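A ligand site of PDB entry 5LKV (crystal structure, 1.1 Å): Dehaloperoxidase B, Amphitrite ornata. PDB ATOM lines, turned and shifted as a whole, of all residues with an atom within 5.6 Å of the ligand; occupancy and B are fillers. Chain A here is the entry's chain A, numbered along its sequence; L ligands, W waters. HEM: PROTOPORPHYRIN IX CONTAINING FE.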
ATOM      1  N   PHE A  24      27.359 -31.035  -0.518  1.00  0.00           N
ATOM      2  CA  PHE A  24      27.051 -30.407  -1.810  1.00  0.00           C
ATOM      3  C   PHE A  24      28.233 -29.627  -2.378  1.00  0.00           C
ATOM      4  O   PHE A  24      28.627 -29.835  -3.532  1.00  0.00           O
ATOM      5  CB  PHE A  24      25.810 -29.497  -1.616  1.00  0.00           C
ATOM      6  CG  PHE A  24      25.559 -28.532  -2.725  1.00  0.00           C
ATOM      7  CD1 PHE A  24      25.179 -28.981  -3.997  1.00  0.00           C
ATOM      8  CD2 PHE A  24      25.679 -27.174  -2.517  1.00  0.00           C
ATOM      9  CE1 PHE A  24      24.913 -28.073  -5.012  1.00  0.00           C
ATOM     10  CE2 PHE A  24      25.415 -26.266  -3.541  1.00  0.00           C
ATOM     11  CZ  PHE A  24      25.026 -26.735  -4.784  1.00  0.00           C
ATOM     12  N   GLU A  31      29.974 -25.054  -7.760  1.00  0.00           N
ATOM     13  CA  GLU A  31      28.809 -24.396  -7.180  1.00  0.00           C
ATOM     14  C   GLU A  31      29.221 -23.307  -6.213  1.00  0.00           C
ATOM     15  O   GLU A  31      28.402 -22.430  -5.886  1.00  0.00           O
ATOM     16  CB  GLU A  31      27.878 -25.420  -6.549  1.00  0.00           C
ATOM     17  CG  GLU A  31      27.211 -26.331  -7.565  1.00  0.00           C
ATOM     18  CD  GLU A  31      26.176 -25.624  -8.416  1.00  0.00           C
ATOM     19  OE1 GLU A  31      26.233 -25.710  -9.673  1.00  0.00           O
ATOM     20  OE2 GLU A  31      25.315 -24.938  -7.848  1.00  0.00           O
ATOM     21  N   ASN A  34      28.565 -19.373  -6.473  1.00  0.00           N
ATOM     22  CA  ASN A  34      27.406 -18.718  -5.880  1.00  0.00           C
ATOM     23  C   ASN A  34      27.640 -18.301  -4.440  1.00  0.00           C
ATOM     24  O   ASN A  34      26.773 -17.646  -3.872  1.00  0.00           O
ATOM     25  CB  ASN A  34      26.215 -19.688  -5.921  1.00  0.00           C
ATOM     26  CG  ASN A  34      25.892 -20.167  -7.300  1.00  0.00           C
ATOM     27  OD1 ASN A  34      25.345 -19.389  -8.047  1.00  0.00           O
ATOM     28  ND2 ASN A  34      26.226 -21.403  -7.669  1.00  0.00           N
ATOM     29  N   PHE A  35      28.782 -18.701  -3.870  1.00  0.00           N
ATOM     30  CA  PHE A  35      29.083 -18.550  -2.455  1.00  0.00           C
ATOM     31  C   PHE A  35      30.558 -18.147  -2.329  1.00  0.00           C
ATOM     32  O   PHE A  35      31.358 -18.850  -1.719  1.00  0.00           O
ATOM     33  CB  PHE A  35      28.826 -19.847  -1.691  1.00  0.00           C
ATOM     34  CG  PHE A  35      27.420 -20.352  -1.831  1.00  0.00           C
ATOM     35  CD1 PHE A  35      26.391 -19.799  -1.085  1.00  0.00           C
ATOM     36  CD2 PHE A  35      27.117 -21.392  -2.693  1.00  0.00           C
ATOM     37  CE1 PHE A  35      25.081 -20.296  -1.217  1.00  0.00           C
ATOM     38  CE2 PHE A  35      25.823 -21.863  -2.832  1.00  0.00           C
ATOM     39  CZ  PHE A  35      24.814 -21.320  -2.090  1.00  0.00           C
ATOM     40  N   TYR A  38      32.879 -18.345   0.691  1.00  0.00           N
ATOM     41  CA  TYR A  38      33.277 -19.658   1.218  1.00  0.00           C
ATOM     42  C   TYR A  38      34.454 -20.276   0.492  1.00  0.00           C
ATOM     43  O   TYR A  38      34.879 -21.362   0.843  1.00  0.00           O
ATOM     44  CB  TYR A  38      32.067 -20.613   1.254  1.00  0.00           C
ATOM     45  CG  TYR A  38      30.872 -20.069   2.021  1.00  0.00           C
ATOM     46  CD1 TYR A  38      31.018 -19.170   3.086  1.00  0.00           C
ATOM     47  CD2 TYR A  38      29.587 -20.462   1.702  1.00  0.00           C
ATOM     48  CE1 TYR A  38      29.944 -18.646   3.778  1.00  0.00           C
ATOM     49  CE2 TYR A  38      28.488 -19.924   2.385  1.00  0.00           C
ATOM     50  CZ  TYR A  38      28.680 -18.988   3.409  1.00  0.00           C
ATOM     51  OH  TYR A  38      27.628 -18.429   4.094  1.00  0.00           O
ATOM     52  N   ASP A  54      24.881 -19.564  10.212  1.00  0.00           N
ATOM     53  CA  ASP A  54      23.588 -18.908  10.407  1.00  0.00           C
ATOM     54  C   ASP A  54      22.748 -18.990   9.114  1.00  0.00           C
ATOM     55  O   ASP A  54      21.558 -19.327   9.156  1.00  0.00           O
ATOM     56  CB  ASP A  54      23.792 -17.441  10.812  1.00  0.00           C
ATOM     57  CG  ASP A  54      24.286 -17.289  12.255  1.00  0.00           C
ATOM     58  OD1 ASP A  54      24.108 -18.204  13.070  1.00  0.00           O
ATOM     59  OD2 ASP A  54      24.818 -16.215  12.578  1.00  0.00           O
ATOM     60  N   HIS A  55      23.357 -18.678   7.970  1.00  0.00           N
ATOM     61  CA  HIS A  55      22.637 -18.733   6.712  1.00  0.00           C
ATOM     62  C   HIS A  55      22.246 -20.147   6.382  1.00  0.00           C
ATOM     63  O   HIS A  55      21.112 -20.403   5.943  1.00  0.00           O
ATOM     64  CB  HIS A  55      23.420 -18.117   5.570  1.00  0.00           C
ATOM     65  CG  HIS A  55      23.625 -16.629   5.732  1.00  0.00           C
ATOM     66  ND1 HIS A  55      24.278 -15.853   4.801  1.00  0.00           N
ATOM     67  CD2 HIS A  55      23.350 -15.784   6.765  1.00  0.00           C
ATOM     68  CE1 HIS A  55      24.263 -14.588   5.183  1.00  0.00           C
ATOM     69  NE2 HIS A  55      23.716 -14.530   6.374  1.00  0.00           N
ATOM     70  N   LYS A  58      19.314 -21.290   8.299  1.00  0.00           N
ATOM     71  CA  LYS A  58      18.089 -20.666   7.836  1.00  0.00           C
ATOM     72  C   LYS A  58      17.604 -21.317   6.523  1.00  0.00           C
ATOM     73  O   LYS A  58      16.391 -21.476   6.325  1.00  0.00           O
ATOM     74  CB  LYS A  58      18.267 -19.172   7.706  1.00  0.00           C
ATOM     75  CG  LYS A  58      18.220 -18.471   9.060  1.00  0.00           C
ATOM     76  CD  LYS A  58      18.661 -17.034   8.973  1.00  0.00           C
ATOM     77  CE  LYS A  58      18.691 -16.324  10.288  1.00  0.00           C
ATOM     78  NZ  LYS A  58      19.409 -15.008  10.243  1.00  0.00           N
ATOM     79  N   VAL A  59      18.516 -21.687   5.645  1.00  0.00           N
ATOM     80  CA  VAL A  59      18.171 -22.416   4.423  1.00  0.00           C
ATOM     81  C   VAL A  59      17.402 -23.690   4.785  1.00  0.00           C
ATOM     82  O   VAL A  59      16.346 -23.995   4.216  1.00  0.00           O
ATOM     83  CB  VAL A  59      19.437 -22.771   3.643  1.00  0.00           C
ATOM     84  CG1 VAL A  59      19.150 -23.786   2.532  1.00  0.00           C
ATOM     85  CG2 VAL A  59      20.072 -21.514   3.094  1.00  0.00           C
ATOM     86  N   PHE A  60      17.980 -24.486   5.689  1.00  0.00           N
ATOM     87  CA  PHE A  60      17.363 -25.746   6.045  1.00  0.00           C
ATOM     88  C   PHE A  60      16.105 -25.568   6.870  1.00  0.00           C
ATOM     89  O   PHE A  60      15.189 -26.390   6.778  1.00  0.00           O
ATOM     90  CB  PHE A  60      18.377 -26.694   6.686  1.00  0.00           C
ATOM     91  CG  PHE A  60      19.218 -27.395   5.640  1.00  0.00           C
ATOM     92  CD1 PHE A  60      20.199 -26.703   4.933  1.00  0.00           C
ATOM     93  CD2 PHE A  60      18.992 -28.711   5.292  1.00  0.00           C
ATOM     94  CE1 PHE A  60      20.956 -27.323   3.950  1.00  0.00           C
ATOM     95  CE2 PHE A  60      19.753 -29.343   4.312  1.00  0.00           C
ATOM     96  CZ  PHE A  60      20.722 -28.649   3.642  1.00  0.00           C
ATOM     97  N   LEU A  62      13.880 -23.330   6.271  1.00  0.00           N
ATOM     98  CA  LEU A  62      12.886 -23.154   5.237  1.00  0.00           C
ATOM     99  C   LEU A  62      12.672 -24.435   4.429  1.00  0.00           C
ATOM    100  O   LEU A  62      11.536 -24.803   4.133  1.00  0.00           O
ATOM    101  CB  LEU A  62      13.267 -21.995   4.312  1.00  0.00           C
ATOM    102  CG  LEU A  62      12.288 -21.706   3.170  1.00  0.00           C
ATOM    103  CD1 LEU A  62      10.870 -21.463   3.669  1.00  0.00           C
ATOM    104  CD2 LEU A  62      12.777 -20.541   2.320  1.00  0.00           C
ATOM    105  N   MET A  63      13.767 -25.135   4.091  1.00  0.00           N
ATOM    106  CA  MET A  63      13.623 -26.378   3.344  1.00  0.00           C
ATOM    107  C   MET A  63      12.698 -27.347   4.078  1.00  0.00           C
ATOM    108  O   MET A  63      11.881 -28.026   3.440  1.00  0.00           O
ATOM    109  CB  MET A  63      14.974 -27.037   3.115  1.00  0.00           C
ATOM    110  CG  MET A  63      14.900 -28.193   2.132  1.00  0.00           C
ATOM    111  SD  MET A  63      16.357 -29.272   2.111  1.00  0.00           S
ATOM    112  CE  MET A  63      17.579 -28.144   1.448  1.00  0.00           C
ATOM    113  N   VAL A  66       9.120 -26.331   3.655  1.00  0.00           N
ATOM    114  CA  VAL A  66       8.629 -26.674   2.320  1.00  0.00           C
ATOM    115  C   VAL A  66       8.330 -28.165   2.223  1.00  0.00           C
ATOM    116  O   VAL A  66       7.296 -28.598   1.701  1.00  0.00           O
ATOM    117  CB  VAL A  66       9.623 -26.214   1.254  1.00  0.00           C
ATOM    118  CG1 VAL A  66       9.180 -26.655  -0.133  1.00  0.00           C
ATOM    119  CG2 VAL A  66       9.781 -24.692   1.294  1.00  0.00           C
ATOM    120  N   LEU A  83      10.745 -19.463  -3.534  1.00  0.00           N
ATOM    121  CA  LEU A  83      12.139 -19.813  -3.823  1.00  0.00           C
ATOM    122  C   LEU A  83      12.650 -19.236  -5.131  1.00  0.00           C
ATOM    123  O   LEU A  83      13.831 -18.899  -5.249  1.00  0.00           O
ATOM    124  CB  LEU A  83      12.307 -21.323  -3.827  1.00  0.00           C
ATOM    125  CG  LEU A  83      12.096 -21.988  -2.462  1.00  0.00           C
ATOM    126  CD1 LEU A  83      11.976 -23.499  -2.596  1.00  0.00           C
ATOM    127  CD2 LEU A  83      13.265 -21.681  -1.533  1.00  0.00           C
ATOM    128  N   MET A  86      12.720 -14.965  -4.433  1.00  0.00           N
ATOM    129  CA  MET A  86      13.596 -14.370  -3.446  1.00  0.00           C
ATOM    130  C   MET A  86      14.824 -13.739  -4.105  1.00  0.00           C
ATOM    131  O   MET A  86      15.436 -14.365  -4.954  1.00  0.00           O
ATOM    132  CB  MET A  86      13.940 -15.294  -2.302  1.00  0.00           C
ATOM    133  CG  MET A  86      14.339 -16.693  -2.597  1.00  0.00           C
ATOM    134  SD  MET A  86      14.219 -17.667  -1.047  1.00  0.00           S
ATOM    135  CE  MET A  86      15.785 -17.169  -0.354  1.00  0.00           C
ATOM    136  N   GLN A  88      17.786 -13.277  -3.187  1.00  0.00           N
ATOM    137  CA  GLN A  88      19.023 -14.004  -3.017  1.00  0.00           C
ATOM    138  C   GLN A  88      19.204 -15.127  -4.039  1.00  0.00           C
ATOM    139  O   GLN A  88      20.309 -15.622  -4.229  1.00  0.00           O
ATOM    140  CB  GLN A  88      19.061 -14.638  -1.640  1.00  0.00           C
ATOM    141  CG  GLN A  88      18.963 -13.644  -0.510  1.00  0.00           C
ATOM    142  CD  GLN A  88      17.558 -13.630   0.081  1.00  0.00           C
ATOM    143  OE1 GLN A  88      16.514 -13.569  -0.645  1.00  0.00           O
ATOM    144  NE2 GLN A  88      17.505 -13.742   1.395  1.00  0.00           N
ATOM    145  N   HIS A  89      18.098 -15.548  -4.678  1.00  0.00           N
ATOM    146  CA  HIS A  89      18.128 -16.586  -5.679  1.00  0.00           C
ATOM    147  C   HIS A  89      18.093 -16.084  -7.098  1.00  0.00           C
ATOM    148  O   HIS A  89      17.931 -16.873  -8.050  1.00  0.00           O
ATOM    149  CB  HIS A  89      16.970 -17.565  -5.416  1.00  0.00           C
ATOM    150  CG  HIS A  89      17.175 -18.415  -4.203  1.00  0.00           C
ATOM    151  ND1 HIS A  89      16.196 -19.246  -3.716  1.00  0.00           N
ATOM    152  CD2 HIS A  89      18.268 -18.628  -3.441  1.00  0.00           C
ATOM    153  CE1 HIS A  89      16.694 -19.913  -2.688  1.00  0.00           C
ATOM    154  NE2 HIS A  89      17.938 -19.557  -2.484  1.00  0.00           N
ATOM    155  N   LEU A  92      19.845 -17.909 -10.282  1.00  0.00           N
ATOM    156  CA  LEU A  92      19.950 -19.374 -10.171  1.00  0.00           C
ATOM    157  C   LEU A  92      19.156 -20.023 -11.276  1.00  0.00           C
ATOM    158  O   LEU A  92      18.224 -19.439 -11.824  1.00  0.00           O
ATOM    159  CB  LEU A  92      19.440 -19.887  -8.836  1.00  0.00           C
ATOM    160  CG  LEU A  92      20.228 -19.367  -7.641  1.00  0.00           C
ATOM    161  CD1 LEU A  92      19.703 -20.012  -6.365  1.00  0.00           C
ATOM    162  CD2 LEU A  92      21.751 -19.576  -7.711  1.00  0.00           C
ATOM    163  N   ASN A  96      21.079 -25.886 -10.251  1.00  0.00           N
ATOM    164  CA  ASN A  96      21.663 -25.645  -8.932  1.00  0.00           C
ATOM    165  C   ASN A  96      20.934 -26.495  -7.863  1.00  0.00           C
ATOM    166  O   ASN A  96      21.531 -27.097  -6.987  1.00  0.00           O
ATOM    167  CB  ASN A  96      21.621 -24.151  -8.564  1.00  0.00           C
ATOM    168  CG  ASN A  96      22.400 -23.258  -9.506  1.00  0.00           C
ATOM    169  OD1 ASN A  96      21.826 -22.456 -10.241  1.00  0.00           O
ATOM    170  ND2 ASN A  96      23.706 -23.377  -9.491  1.00  0.00           N
ATOM    171  N   PHE A  97      19.616 -26.475  -7.958  1.00  0.00           N
ATOM    172  CA  PHE A  97      18.751 -27.200  -7.023  1.00  0.00           C
ATOM    173  C   PHE A  97      18.853 -28.703  -7.236  1.00  0.00           C
ATOM    174  O   PHE A  97      18.862 -29.479  -6.268  1.00  0.00           O
ATOM    175  CB  PHE A  97      17.290 -26.713  -7.152  1.00  0.00           C
ATOM    176  CG  PHE A  97      17.085 -25.319  -6.639  1.00  0.00           C
ATOM    177  CD1 PHE A  97      17.438 -24.204  -7.412  1.00  0.00           C
ATOM    178  CD2 PHE A  97      16.554 -25.106  -5.391  1.00  0.00           C
ATOM    179  CE1 PHE A  97      17.295 -22.942  -6.902  1.00  0.00           C
ATOM    180  CE2 PHE A  97      16.386 -23.830  -4.890  1.00  0.00           C
ATOM    181  CZ  PHE A  97      16.752 -22.746  -5.647  1.00  0.00           C
ATOM    182  N   LEU A 100      21.980 -29.860  -5.454  1.00  0.00           N
ATOM    183  CA  LEU A 100      21.838 -29.847  -4.030  1.00  0.00           C
ATOM    184  C   LEU A 100      21.112 -31.119  -3.550  1.00  0.00           C
ATOM    185  O   LEU A 100      21.535 -31.755  -2.568  1.00  0.00           O
ATOM    186  CB  LEU A 100      21.099 -28.584  -3.579  1.00  0.00           C
ATOM    187  CG  LEU A 100      20.769 -28.504  -2.092  1.00  0.00           C
ATOM    188  CD1 LEU A 100      22.006 -28.539  -1.234  1.00  0.00           C
ATOM    189  CD2 LEU A 100      19.954 -27.241  -1.832  1.00  0.00           C
ATOM    190  N   PHE A 101      20.029 -31.492  -4.217  1.00  0.00           N
ATOM    191  CA  PHE A 101      19.274 -32.664  -3.805  1.00  0.00           C
ATOM    192  C   PHE A 101      19.981 -33.969  -4.127  1.00  0.00           C
ATOM    193  O   PHE A 101      19.844 -34.922  -3.350  1.00  0.00           O
ATOM    194  CB  PHE A 101      17.806 -32.582  -4.266  1.00  0.00           C
ATOM    195  CG  PHE A 101      17.041 -31.634  -3.403  1.00  0.00           C
ATOM    196  CD1 PHE A 101      16.486 -32.087  -2.222  1.00  0.00           C
ATOM    197  CD2 PHE A 101      16.969 -30.292  -3.694  1.00  0.00           C
ATOM    198  CE1 PHE A 101      15.907 -31.200  -1.339  1.00  0.00           C
ATOM    199  CE2 PHE A 101      16.370 -29.395  -2.807  1.00  0.00           C
ATOM    200  CZ  PHE A 101      15.830 -29.867  -1.632  1.00  0.00           C
ATOM    201  N   LEU A 127      10.475 -30.644  -6.596  1.00  0.00           N
ATOM    202  CA  LEU A 127      10.753 -29.246  -6.342  1.00  0.00           C
ATOM    203  C   LEU A 127      11.310 -28.595  -7.599  1.00  0.00           C
ATOM    204  O   LEU A 127      10.874 -27.523  -7.974  1.00  0.00           O
ATOM    205  CB  LEU A 127      11.721 -29.107  -5.160  1.00  0.00           C
ATOM    206  CG  LEU A 127      12.118 -27.660  -4.862  1.00  0.00           C
ATOM    207  CD1 LEU A 127      10.914 -26.782  -4.518  1.00  0.00           C
ATOM    208  CD2 LEU A 127      13.150 -27.635  -3.767  1.00  0.00           C
HETATM  209  CHA HEM L   1      20.110 -17.521   0.370  1.00  0.00           C
HETATM  210  CHB HEM L   1      16.810 -20.987   1.072  1.00  0.00           C
HETATM  211  CHC HEM L   1      18.674 -23.511  -2.586  1.00  0.00           C
HETATM  212  CHD HEM L   1      21.861 -19.967  -3.391  1.00  0.00           C
HETATM  213  C1A HEM L   1      19.085 -18.299   0.902  1.00  0.00           C
HETATM  214  C2A HEM L   1      18.373 -17.933   2.084  1.00  0.00           C
HETATM  215  C3A HEM L   1      17.439 -18.907   2.290  1.00  0.00           C
HETATM  216  C4A HEM L   1      17.584 -19.818   1.222  1.00  0.00           C
HETATM  217  CMA HEM L   1      16.418 -18.986   3.406  1.00  0.00           C
HETATM  218  CAA HEM L   1      18.675 -16.751   3.000  1.00  0.00           C
HETATM  219  CBA HEM L   1      19.827 -17.145   3.960  1.00  0.00           C
HETATM  220  CGA HEM L   1      20.246 -15.995   4.831  1.00  0.00           C
HETATM  221  O1A HEM L   1      20.999 -15.122   4.376  1.00  0.00           O
HETATM  222  O2A HEM L   1      19.985 -16.015   6.031  1.00  0.00           O
HETATM  223  C1B HEM L   1      17.042 -21.986   0.130  1.00  0.00           C
HETATM  224  C2B HEM L   1      16.280 -23.214   0.061  1.00  0.00           C
HETATM  225  C3B HEM L   1      16.803 -23.938  -0.955  1.00  0.00           C
HETATM  226  C4B HEM L   1      17.897 -23.136  -1.510  1.00  0.00           C
HETATM  227  CMB HEM L   1      15.214 -23.638   1.018  1.00  0.00           C
HETATM  228  CAB HEM L   1      16.446 -25.274  -1.468  1.00  0.00           C
HETATM  229  CBB HEM L   1      15.222 -25.825  -1.349  1.00  0.00           C
HETATM  230  C1C HEM L   1      19.717 -22.775  -3.131  1.00  0.00           C
HETATM  231  C2C HEM L   1      20.600 -23.254  -4.126  1.00  0.00           C
HETATM  232  C3C HEM L   1      21.543 -22.262  -4.331  1.00  0.00           C
HETATM  233  C4C HEM L   1      21.193 -21.163  -3.475  1.00  0.00           C
HETATM  234  CMC HEM L   1      20.476 -24.579  -4.819  1.00  0.00           C
HETATM  235  CAC HEM L   1      22.725 -22.285  -5.211  1.00  0.00           C
HETATM  236  CBC HEM L   1      23.409 -23.389  -5.502  1.00  0.00           C
HETATM  237  C1D HEM L   1      21.605 -18.987  -2.477  1.00  0.00           C
HETATM  238  C2D HEM L   1      22.416 -17.776  -2.371  1.00  0.00           C
HETATM  239  C3D HEM L   1      21.964 -17.105  -1.297  1.00  0.00           C
HETATM  240  C4D HEM L   1      20.833 -17.875  -0.756  1.00  0.00           C
HETATM  241  CMD HEM L   1      23.570 -17.414  -3.265  1.00  0.00           C
HETATM  242  CAD HEM L   1      22.506 -15.795  -0.777  1.00  0.00           C
HETATM  243  CBD HEM L   1      23.589 -16.065   0.301  1.00  0.00           C
HETATM  244  CGD HEM L   1      22.903 -16.244   1.664  1.00  0.00           C
HETATM  245  O1D HEM L   1      22.082 -15.349   2.062  1.00  0.00           O
HETATM  246  O2D HEM L   1      23.116 -17.240   2.322  1.00  0.00           O
HETATM  247  NA  HEM L   1      18.606 -19.459   0.360  1.00  0.00           N
HETATM  248  NB  HEM L   1      17.992 -21.964  -0.835  1.00  0.00           N
HETATM  249  NC  HEM L   1      20.093 -21.515  -2.754  1.00  0.00           N
HETATM  250  ND  HEM L   1      20.645 -18.993  -1.526  1.00  0.00           N
HETATM  251 FE   HEM L   1      19.318 -20.453  -1.209  1.00  0.00          FE
HETATM  252  O   HOH W   1      26.017 -15.448   2.763  1.00  0.00           O
HETATM  253  O   HOH W   2      25.464 -18.632   2.430  1.00  0.00           O
HETATM  254  O   HOH W   3      20.030 -13.954   7.742  1.00  0.00           O
HETATM  255  O   HOH W   4      22.478 -12.607   1.170  1.00  0.00           O
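Water W3 bridges O2A of the ligand and NZ of Lys 58.
Water W2 bridges an oxygen (O2D) of the ligand (2.7 Å) and the side-chain hydroxyl of Tyr 38 (2.7 Å).
Water W1 bridges ND1 of His 55 and O2D of the ligand.
NE2 of His 89 is bound to FE of the ligand (2.1 Å).
ND1 of His 55 lies within hydrogen-bond range of O2D of the ligand.
Residues that only touch the ligand: Phe 97, Asn 34, Lys 58, Glu 31, Val 59, Leu 92, Asn 96, Phe 35, Gln 88, Met 86, Leu 127, Met 63, Leu 83 and Phe 24.
Hydrophobic or aromatic side chains that line the ligand: Phe 24, Phe 35, His 55, Val 59, Leu 83, Met 86, His 89, Leu 92, Phe 97 and Leu 127.
ND1 of His 89 sits close to SD of Met 86 (3.7 Å).
ND2 of Asn 34 sits at hydrogen-bond distance from O of Glu 31 (3.0 Å).
The side-chain carboxylate (OE2) of Glu 31 sits at hydrogen-bond distance from the side-chain amide nitrogen (ND2) of Asn 96, 2.8 Å away.
The backbone carbonyl oxygen (O) of Leu 83 sits at hydrogen-bond distance from a ring nitrogen (ND1) of His 89 (2.8 Å).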
